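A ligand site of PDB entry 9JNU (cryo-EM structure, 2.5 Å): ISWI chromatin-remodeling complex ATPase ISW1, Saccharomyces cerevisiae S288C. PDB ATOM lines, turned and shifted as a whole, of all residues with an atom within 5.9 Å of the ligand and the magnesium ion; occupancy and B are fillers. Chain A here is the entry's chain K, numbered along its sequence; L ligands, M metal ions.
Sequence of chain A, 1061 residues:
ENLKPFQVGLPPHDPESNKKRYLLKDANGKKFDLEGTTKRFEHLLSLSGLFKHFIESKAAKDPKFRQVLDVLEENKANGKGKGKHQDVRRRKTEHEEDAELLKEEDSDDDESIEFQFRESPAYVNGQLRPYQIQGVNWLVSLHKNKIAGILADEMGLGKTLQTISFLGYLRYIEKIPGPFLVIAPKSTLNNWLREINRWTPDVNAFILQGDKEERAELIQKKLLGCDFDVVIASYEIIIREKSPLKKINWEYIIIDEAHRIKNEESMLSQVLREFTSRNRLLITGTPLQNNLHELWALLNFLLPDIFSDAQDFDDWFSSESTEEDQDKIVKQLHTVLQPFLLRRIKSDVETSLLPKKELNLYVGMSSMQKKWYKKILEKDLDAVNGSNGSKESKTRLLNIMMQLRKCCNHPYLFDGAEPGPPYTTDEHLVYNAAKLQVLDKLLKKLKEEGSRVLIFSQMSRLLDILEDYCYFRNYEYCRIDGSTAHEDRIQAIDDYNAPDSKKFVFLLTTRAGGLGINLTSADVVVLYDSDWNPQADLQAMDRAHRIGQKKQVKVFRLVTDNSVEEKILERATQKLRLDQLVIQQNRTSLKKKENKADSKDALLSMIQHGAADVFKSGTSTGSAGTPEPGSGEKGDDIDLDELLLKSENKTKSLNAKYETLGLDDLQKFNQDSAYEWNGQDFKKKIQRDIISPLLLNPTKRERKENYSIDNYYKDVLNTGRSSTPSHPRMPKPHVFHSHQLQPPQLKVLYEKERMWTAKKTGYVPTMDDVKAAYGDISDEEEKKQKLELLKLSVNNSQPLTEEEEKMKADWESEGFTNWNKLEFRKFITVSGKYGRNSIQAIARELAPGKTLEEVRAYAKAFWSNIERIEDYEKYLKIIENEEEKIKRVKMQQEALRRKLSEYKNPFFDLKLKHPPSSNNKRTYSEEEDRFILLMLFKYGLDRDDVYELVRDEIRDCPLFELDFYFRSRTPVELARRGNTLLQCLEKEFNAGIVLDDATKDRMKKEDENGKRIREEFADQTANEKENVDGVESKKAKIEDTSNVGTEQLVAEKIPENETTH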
ATOM      1  N   GLN A 127     -18.777 -10.801   2.215  1.00  0.00           N
ATOM      2  CA  GLN A 127     -19.354 -12.094   2.551  1.00  0.00           C
ATOM      3  C   GLN A 127     -18.372 -13.203   2.203  1.00  0.00           C
ATOM      4  O   GLN A 127     -17.429 -13.010   1.427  1.00  0.00           O
ATOM      5  CB  GLN A 127     -20.680 -12.304   1.798  1.00  0.00           C
ATOM      6  CG  GLN A 127     -21.910 -11.950   2.621  1.00  0.00           C
ATOM      7  CD  GLN A 127     -22.390 -13.100   3.472  1.00  0.00           C
ATOM      8  OE1 GLN A 127     -22.026 -14.254   3.236  1.00  0.00           O
ATOM      9  NE2 GLN A 127     -23.207 -12.798   4.475  1.00  0.00           N
ATOM     10  N   LEU A 128     -18.600 -14.382   2.769  1.00  0.00           N
ATOM     11  CA  LEU A 128     -17.737 -15.529   2.509  1.00  0.00           C
ATOM     12  C   LEU A 128     -18.586 -16.768   2.269  1.00  0.00           C
ATOM     13  O   LEU A 128     -19.771 -16.814   2.595  1.00  0.00           O
ATOM     14  CB  LEU A 128     -16.725 -15.734   3.654  1.00  0.00           C
ATOM     15  CG  LEU A 128     -17.100 -15.531   5.125  1.00  0.00           C
ATOM     16  CD1 LEU A 128     -18.141 -16.524   5.580  1.00  0.00           C
ATOM     17  CD2 LEU A 128     -15.865 -15.593   6.025  1.00  0.00           C
ATOM     18  N   ARG A 129     -17.944 -17.779   1.692  1.00  0.00           N
ATOM     19  CA  ARG A 129     -18.648 -18.939   1.177  1.00  0.00           C
ATOM     20  C   ARG A 129     -19.208 -19.804   2.312  1.00  0.00           C
ATOM     21  O   ARG A 129     -18.677 -19.796   3.427  1.00  0.00           O
ATOM     22  CB  ARG A 129     -17.705 -19.756   0.294  1.00  0.00           C
ATOM     23  CG  ARG A 129     -16.852 -18.849  -0.583  1.00  0.00           C
ATOM     24  CD  ARG A 129     -15.891 -19.606  -1.468  1.00  0.00           C
ATOM     25  NE  ARG A 129     -14.952 -18.700  -2.126  1.00  0.00           N
ATOM     26  CZ  ARG A 129     -13.703 -18.485  -1.722  1.00  0.00           C
ATOM     27  NH1 ARG A 129     -13.241 -19.125  -0.654  1.00  0.00           N
ATOM     28  NH2 ARG A 129     -12.931 -17.641  -2.371  1.00  0.00           N
ATOM     29  N   GLN A 132     -17.111 -21.857   4.649  1.00  0.00           N
ATOM     30  CA  GLN A 132     -16.356 -21.036   5.589  1.00  0.00           C
ATOM     31  C   GLN A 132     -17.190 -20.719   6.822  1.00  0.00           C
ATOM     32  O   GLN A 132     -16.683 -20.720   7.951  1.00  0.00           O
ATOM     33  CB  GLN A 132     -15.864 -19.769   4.907  1.00  0.00           C
ATOM     34  CG  GLN A 132     -14.701 -20.007   3.973  1.00  0.00           C
ATOM     35  CD  GLN A 132     -14.500 -18.870   2.981  1.00  0.00           C
ATOM     36  OE1 GLN A 132     -15.423 -18.483   2.271  1.00  0.00           O
ATOM     37  NE2 GLN A 132     -13.276 -18.345   2.941  1.00  0.00           N
ATOM     38  N   GLU A 154      -8.171 -28.169   2.481  1.00  0.00           N
ATOM     39  CA  GLU A 154      -7.141 -28.261   1.454  1.00  0.00           C
ATOM     40  C   GLU A 154      -6.665 -26.877   1.059  1.00  0.00           C
ATOM     41  O   GLU A 154      -7.398 -25.890   1.170  1.00  0.00           O
ATOM     42  CB  GLU A 154      -7.651 -29.025   0.239  1.00  0.00           C
ATOM     43  CG  GLU A 154      -7.759 -30.522   0.471  1.00  0.00           C
ATOM     44  CD  GLU A 154      -8.548 -31.208  -0.620  1.00  0.00           C
ATOM     45  OE1 GLU A 154      -9.106 -30.509  -1.477  1.00  0.00           O
ATOM     46  OE2 GLU A 154      -8.617 -32.462  -0.600  1.00  0.00           O
ATOM     47  N   MET A 155      -5.425 -26.813   0.598  1.00  0.00           N
ATOM     48  CA  MET A 155      -4.800 -25.542   0.251  1.00  0.00           C
ATOM     49  C   MET A 155      -5.611 -24.796  -0.802  1.00  0.00           C
ATOM     50  O   MET A 155      -6.062 -25.393  -1.792  1.00  0.00           O
ATOM     51  CB  MET A 155      -3.378 -25.768  -0.242  1.00  0.00           C
ATOM     52  CG  MET A 155      -2.668 -24.520  -0.719  1.00  0.00           C
ATOM     53  SD  MET A 155      -1.880 -24.739  -2.324  1.00  0.00           S
ATOM     54  CE  MET A 155      -3.296 -24.665  -3.416  1.00  0.00           C
ATOM     55  N   GLY A 156      -5.815 -23.502  -0.585  1.00  0.00           N
ATOM     56  CA  GLY A 156      -6.532 -22.658  -1.503  1.00  0.00           C
ATOM     57  C   GLY A 156      -8.004 -22.473  -1.189  1.00  0.00           C
ATOM     58  O   GLY A 156      -8.624 -21.550  -1.727  1.00  0.00           O
ATOM     59  N   LEU A 157      -8.574 -23.318  -0.331  1.00  0.00           N
ATOM     60  CA  LEU A 157      -9.964 -23.145   0.055  1.00  0.00           C
ATOM     61  C   LEU A 157     -10.171 -21.852   0.820  1.00  0.00           C
ATOM     62  O   LEU A 157     -11.263 -21.264   0.769  1.00  0.00           O
ATOM     63  CB  LEU A 157     -10.434 -24.338   0.890  1.00  0.00           C
ATOM     64  CG  LEU A 157     -10.550 -25.671   0.166  1.00  0.00           C
ATOM     65  CD1 LEU A 157     -11.033 -26.747   1.117  1.00  0.00           C
ATOM     66  CD2 LEU A 157     -11.478 -25.559  -1.027  1.00  0.00           C
ATOM     67  N   GLY A 158      -9.142 -21.389   1.520  1.00  0.00           N
ATOM     68  CA  GLY A 158      -9.227 -20.179   2.299  1.00  0.00           C
ATOM     69  C   GLY A 158      -9.399 -20.499   3.766  1.00  0.00           C
ATOM     70  O   GLY A 158     -10.517 -20.753   4.228  1.00  0.00           O
ATOM     71  N   LYS A 159      -8.295 -20.474   4.511  1.00  0.00           N
ATOM     72  CA  LYS A 159      -8.312 -20.754   5.932  1.00  0.00           C
ATOM     73  C   LYS A 159      -7.927 -19.557   6.780  1.00  0.00           C
ATOM     74  O   LYS A 159      -8.387 -19.441   7.918  1.00  0.00           O
ATOM     75  CB  LYS A 159      -7.378 -21.926   6.253  1.00  0.00           C
ATOM     76  CG  LYS A 159      -7.729 -23.209   5.503  1.00  0.00           C
ATOM     77  CD  LYS A 159      -6.864 -24.374   5.959  1.00  0.00           C
ATOM     78  CE  LYS A 159      -5.527 -24.383   5.250  1.00  0.00           C
ATOM     79  NZ  LYS A 159      -4.722 -25.599   5.574  1.00  0.00           N
ATOM     80  N   THR A 160      -7.086 -18.671   6.245  1.00  0.00           N
ATOM     81  CA  THR A 160      -6.750 -17.451   6.965  1.00  0.00           C
ATOM     82  C   THR A 160      -7.992 -16.600   7.195  1.00  0.00           C
ATOM     83  O   THR A 160      -8.159 -16.023   8.275  1.00  0.00           O
ATOM     84  CB  THR A 160      -5.703 -16.660   6.193  1.00  0.00           C
ATOM     85  OG1 THR A 160      -6.265 -16.184   4.961  1.00  0.00           O
ATOM     86  CG2 THR A 160      -4.501 -17.538   5.887  1.00  0.00           C
ATOM     87  N   LEU A 161      -8.868 -16.511   6.194  1.00  0.00           N
ATOM     88  CA  LEU A 161     -10.096 -15.742   6.370  1.00  0.00           C
ATOM     89  C   LEU A 161     -10.963 -16.344   7.470  1.00  0.00           C
ATOM     90  O   LEU A 161     -11.502 -15.607   8.308  1.00  0.00           O
ATOM     91  CB  LEU A 161     -10.878 -15.694   5.055  1.00  0.00           C
ATOM     92  CG  LEU A 161     -12.270 -15.080   5.181  1.00  0.00           C
ATOM     93  CD1 LEU A 161     -12.184 -13.655   5.707  1.00  0.00           C
ATOM     94  CD2 LEU A 161     -13.001 -15.111   3.855  1.00  0.00           C
ATOM     95  N   THR A 188       4.830 -15.927   4.412  1.00  0.00           N
ATOM     96  CA  THR A 188       3.406 -15.617   4.421  1.00  0.00           C
ATOM     97  C   THR A 188       3.021 -14.530   5.425  1.00  0.00           C
ATOM     98  O   THR A 188       1.826 -14.268   5.575  1.00  0.00           O
ATOM     99  CB  THR A 188       2.592 -16.879   4.707  1.00  0.00           C
ATOM    100  OG1 THR A 188       2.754 -17.250   6.082  1.00  0.00           O
ATOM    101  CG2 THR A 188       3.058 -18.022   3.834  1.00  0.00           C
ATOM    102  N   ASN A 191       1.131 -11.640   3.837  1.00  0.00           N
ATOM    103  CA  ASN A 191      -0.208 -12.046   3.441  1.00  0.00           C
ATOM    104  C   ASN A 191      -1.154 -12.090   4.631  1.00  0.00           C
ATOM    105  O   ASN A 191      -2.303 -11.644   4.538  1.00  0.00           O
ATOM    106  CB  ASN A 191      -0.157 -13.402   2.751  1.00  0.00           C
ATOM    107  CG  ASN A 191      -1.486 -13.805   2.139  1.00  0.00           C
ATOM    108  OD1 ASN A 191      -1.768 -13.486   0.986  1.00  0.00           O
ATOM    109  ND2 ASN A 191      -2.303 -14.492   2.919  1.00  0.00           N
ATOM    110  N   TRP A 192      -0.676 -12.610   5.760  1.00  0.00           N
ATOM    111  CA  TRP A 192      -1.490 -12.620   6.983  1.00  0.00           C
ATOM    112  C   TRP A 192      -1.863 -11.203   7.395  1.00  0.00           C
ATOM    113  O   TRP A 192      -3.020 -10.914   7.707  1.00  0.00           O
ATOM    114  CB  TRP A 192      -0.737 -13.320   8.102  1.00  0.00           C
ATOM    115  CG  TRP A 192      -1.104 -14.745   8.312  1.00  0.00           C
ATOM    116  CD1 TRP A 192      -0.394 -15.838   7.908  1.00  0.00           C
ATOM    117  CD2 TRP A 192      -2.269 -15.246   8.967  1.00  0.00           C
ATOM    118  NE1 TRP A 192      -1.040 -16.989   8.283  1.00  0.00           N
ATOM    119  CE2 TRP A 192      -2.197 -16.650   8.931  1.00  0.00           C
ATOM    120  CE3 TRP A 192      -3.366 -14.645   9.588  1.00  0.00           C
ATOM    121  CZ2 TRP A 192      -3.188 -17.463   9.488  1.00  0.00           C
ATOM    122  CZ3 TRP A 192      -4.333 -15.446  10.141  1.00  0.00           C
ATOM    123  CH2 TRP A 192      -4.244 -16.839  10.090  1.00  0.00           C
ATOM    124  N   GLU A 195      -4.449  -9.722   5.003  1.00  0.00           N
ATOM    125  CA  GLU A 195      -5.767 -10.310   5.206  1.00  0.00           C
ATOM    126  C   GLU A 195      -6.431  -9.733   6.448  1.00  0.00           C
ATOM    127  O   GLU A 195      -7.621  -9.392   6.428  1.00  0.00           O
ATOM    128  CB  GLU A 195      -5.632 -11.827   5.312  1.00  0.00           C
ATOM    129  CG  GLU A 195      -6.828 -12.609   4.831  1.00  0.00           C
ATOM    130  CD  GLU A 195      -6.939 -12.591   3.317  1.00  0.00           C
ATOM    131  OE1 GLU A 195      -5.893 -12.425   2.650  1.00  0.00           O
ATOM    132  OE2 GLU A 195      -8.064 -12.758   2.799  1.00  0.00           O
ATOM    133  N   ARG A 198      -7.613  -6.399   5.862  1.00  0.00           N
ATOM    134  CA  ARG A 198      -8.653  -6.337   4.847  1.00  0.00           C
ATOM    135  C   ARG A 198     -10.033  -6.690   5.397  1.00  0.00           C
ATOM    136  O   ARG A 198     -10.982  -5.942   5.190  1.00  0.00           O
ATOM    137  CB  ARG A 198      -8.305  -7.268   3.685  1.00  0.00           C
ATOM    138  CG  ARG A 198      -9.362  -7.299   2.588  1.00  0.00           C
ATOM    139  CD  ARG A 198      -8.968  -8.234   1.460  1.00  0.00           C
ATOM    140  NE  ARG A 198     -10.072  -8.483   0.545  1.00  0.00           N
ATOM    141  CZ  ARG A 198     -10.006  -9.283  -0.504  1.00  0.00           C
ATOM    142  NH1 ARG A 198      -8.880  -9.912  -0.791  1.00  0.00           N
ATOM    143  NH2 ARG A 198     -11.067  -9.462  -1.284  1.00  0.00           N
ATOM    144  N   TRP A 199     -10.160  -7.815   6.106  1.00  0.00           N
ATOM    145  CA  TRP A 199     -11.499  -8.242   6.503  1.00  0.00           C
ATOM    146  C   TRP A 199     -11.955  -7.698   7.849  1.00  0.00           C
ATOM    147  O   TRP A 199     -13.145  -7.440   8.022  1.00  0.00           O
ATOM    148  CB  TRP A 199     -11.597  -9.768   6.522  1.00  0.00           C
ATOM    149  CG  TRP A 199     -11.059 -10.409   5.292  1.00  0.00           C
ATOM    150  CD1 TRP A 199      -9.862 -11.051   5.151  1.00  0.00           C
ATOM    151  CD2 TRP A 199     -11.688 -10.469   4.012  1.00  0.00           C
ATOM    152  NE1 TRP A 199      -9.714 -11.507   3.872  1.00  0.00           N
ATOM    153  CE2 TRP A 199     -10.827 -11.159   3.152  1.00  0.00           C
ATOM    154  CE3 TRP A 199     -12.910  -9.998   3.510  1.00  0.00           C
ATOM    155  CZ2 TRP A 199     -11.134 -11.400   1.811  1.00  0.00           C
ATOM    156  CZ3 TRP A 199     -13.217 -10.232   2.187  1.00  0.00           C
ATOM    157  CH2 TRP A 199     -12.331 -10.932   1.353  1.00  0.00           C
ATOM    158  N   ASP A 256      -0.066 -21.627  11.378  1.00  0.00           N
ATOM    159  CA  ASP A 256      -0.336 -21.977   9.994  1.00  0.00           C
ATOM    160  C   ASP A 256       0.735 -22.952   9.520  1.00  0.00           C
ATOM    161  O   ASP A 256       1.904 -22.820   9.869  1.00  0.00           O
ATOM    162  CB  ASP A 256      -0.362 -20.741   9.109  1.00  0.00           C
ATOM    163  CG  ASP A 256      -0.854 -21.039   7.689  1.00  0.00           C
ATOM    164  OD1 ASP A 256      -1.131 -22.217   7.395  1.00  0.00           O
ATOM    165  OD2 ASP A 256      -0.957 -20.095   6.885  1.00  0.00           O
ATOM    166  N   GLU A 257       0.318 -23.919   8.709  1.00  0.00           N
ATOM    167  CA  GLU A 257       1.178 -25.022   8.270  1.00  0.00           C
ATOM    168  C   GLU A 257       1.778 -25.731   9.487  1.00  0.00           C
ATOM    169  O   GLU A 257       2.986 -25.781   9.694  1.00  0.00           O
ATOM    170  CB  GLU A 257       2.257 -24.528   7.314  1.00  0.00           C
ATOM    171  CG  GLU A 257       1.704 -23.799   6.101  1.00  0.00           C
ATOM    172  CD  GLU A 257       0.574 -24.555   5.428  1.00  0.00           C
ATOM    173  OE1 GLU A 257       0.678 -25.796   5.285  1.00  0.00           O
ATOM    174  OE2 GLU A 257      -0.425 -23.913   5.046  1.00  0.00           O
ATOM    175  N   ILE A 283      -3.411 -25.044  11.877  1.00  0.00           N
ATOM    176  CA  ILE A 283      -3.870 -24.964  10.503  1.00  0.00           C
ATOM    177  C   ILE A 283      -2.843 -25.671   9.632  1.00  0.00           C
ATOM    178  O   ILE A 283      -1.678 -25.266   9.605  1.00  0.00           O
ATOM    179  CB  ILE A 283      -4.058 -23.508  10.043  1.00  0.00           C
ATOM    180  CG1 ILE A 283      -5.041 -22.783  10.941  1.00  0.00           C
ATOM    181  CG2 ILE A 283      -4.528 -23.458   8.606  1.00  0.00           C
ATOM    182  CD1 ILE A 283      -5.085 -21.304  10.701  1.00  0.00           C
ATOM    183  N   LEU A 515       4.745 -22.722  -0.557  1.00  0.00           N
ATOM    184  CA  LEU A 515       3.454 -22.866  -1.194  1.00  0.00           C
ATOM    185  C   LEU A 515       3.037 -21.633  -2.001  1.00  0.00           C
ATOM    186  O   LEU A 515       1.949 -21.638  -2.592  1.00  0.00           O
ATOM    187  CB  LEU A 515       2.378 -23.169  -0.152  1.00  0.00           C
ATOM    188  CG  LEU A 515       2.136 -24.652   0.169  1.00  0.00           C
ATOM    189  CD1 LEU A 515       3.164 -25.157   1.164  1.00  0.00           C
ATOM    190  CD2 LEU A 515       0.729 -24.863   0.683  1.00  0.00           C
HETATM  191  P1  LIG L   1      -3.504 -21.008   3.266  1.00  0.00           P
HETATM  192  O1  LIG L   1      -2.674 -21.297   2.043  1.00  0.00           O
HETATM  193  O2  LIG L   1      -2.697 -20.689   4.502  1.00  0.00           O
HETATM  194  O3  LIG L   1      -4.641 -21.967   3.490  1.00  0.00           O
HETATM  195  P2  LIG L   1      -5.192 -19.515   1.631  1.00  0.00           P
HETATM  196  O4  LIG L   1      -5.687 -20.891   1.270  1.00  0.00           O
HETATM  197  O5  LIG L   1      -4.493 -18.675   0.584  1.00  0.00           O
HETATM  198  O6  LIG L   1      -4.235 -19.619   2.929  1.00  0.00           O
HETATM  199  O7  LIG L   1      -6.452 -18.682   2.178  1.00  0.00           O
HETATM  200  C1  LIG L   1      -6.570 -17.298   1.889  1.00  0.00           C
HETATM  201  C2  LIG L   1      -7.394 -17.233   0.609  1.00  0.00           C
HETATM  202  O8  LIG L   1      -8.670 -16.599   0.773  1.00  0.00           O
HETATM  203  C3  LIG L   1      -6.690 -16.469  -0.483  1.00  0.00           C
HETATM  204  O9  LIG L   1      -5.928 -17.362  -1.286  1.00  0.00           O
HETATM  205  C4  LIG L   1      -7.817 -15.859  -1.296  1.00  0.00           C
HETATM  206  O10 LIG L   1      -7.819 -16.412  -2.615  1.00  0.00           O
HETATM  207  C5  LIG L   1      -9.073 -16.273  -0.558  1.00  0.00           C
HETATM  208  N1  LIG L   1     -10.120 -15.220  -0.619  1.00  0.00           N
HETATM  209  C6  LIG L   1      -9.957 -13.983  -1.124  1.00  0.00           C
HETATM  210  N2  LIG L   1     -11.112 -13.273  -1.063  1.00  0.00           N
HETATM  211  C7  LIG L   1     -12.047 -14.078  -0.519  1.00  0.00           C
HETATM  212  C8  LIG L   1     -13.481 -13.959  -0.167  1.00  0.00           C
HETATM  213  N3  LIG L   1     -14.172 -12.810  -0.388  1.00  0.00           N
HETATM  214  N4  LIG L   1     -14.086 -15.034   0.383  1.00  0.00           N
HETATM  215  C9  LIG L   1     -13.414 -16.178   0.601  1.00  0.00           C
HETATM  216  N5  LIG L   1     -12.113 -16.361   0.314  1.00  0.00           N
HETATM  217  C10 LIG L   1     -11.393 -15.363  -0.246  1.00  0.00           C
HETATM  218 MG    MG M   1      -1.113 -20.889   3.346  1.00  0.00          MG
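NE1 of Trp 192 is in hydrogen-bond range of OD2 of Asp 256, 3.4 Å away.
N of Arg 129 is in hydrogen-bond range of OE1 of Gln 132 (2.7 Å).
NH1 of Arg 129 lies within hydrogen-bond range of O of Leu 157 (3.2 Å).
The backbone NH (N) of Glu 257 is in hydrogen-bond range of the backbone carbonyl oxygen (O) of Ile 283.
The side-chain carboxylate (OD2) of Asp 256 sits close to an oxygen (O2) of the ligand (3.0 Å).
Gln 127 touches the ligand.
OG1 of Thr 160 touches C1 of the ligand, 3.3 Å away.
Leu 161 touches the ligand (CD2 to C9, 3.4 Å).
Arg 198 touches the ligand (NH2 to N2, 3.8 Å).
Trp 199 touches the ligand.
Glu 257 touches the ligand (OE2 to O2, 3.98 Å).
Residues that only touch the magnesium ion: Glu 257 (3.5 Å) and Asp 256 (3.6 Å).
Of the 22 residues printed, 2 come within 4 Å of the magnesium ion.
The nearest printed residue that does not touch the magnesium ion is Thr 188 (5.1 Å).
O2 of the ligand is bound to the magnesium ion (2.0 Å).
An oxygen (O1) of the ligand binds the magnesium ion (2.1 Å).
The magnesium ion has two donor atoms within binding distance.
The backbone NH (N) of Gly 156 is in hydrogen-bond range of an oxygen (O4) of the ligand, at 3.2 Å.
The backbone NH (N) of Lys 159 is in hydrogen-bond range of an oxygen (O7) of the ligand (3.5 Å).
N5 of the ligand is in hydrogen-bond range of NH2 of Arg 129 (3.1 Å).
N of Gly 158 is in hydrogen-bond range of O4 of the ligand (3.5 Å).
The side-chain amide nitrogen (NE2) of Gln 132 lies close to a nitrogen (N5) of the ligand, 3.5 Å away.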
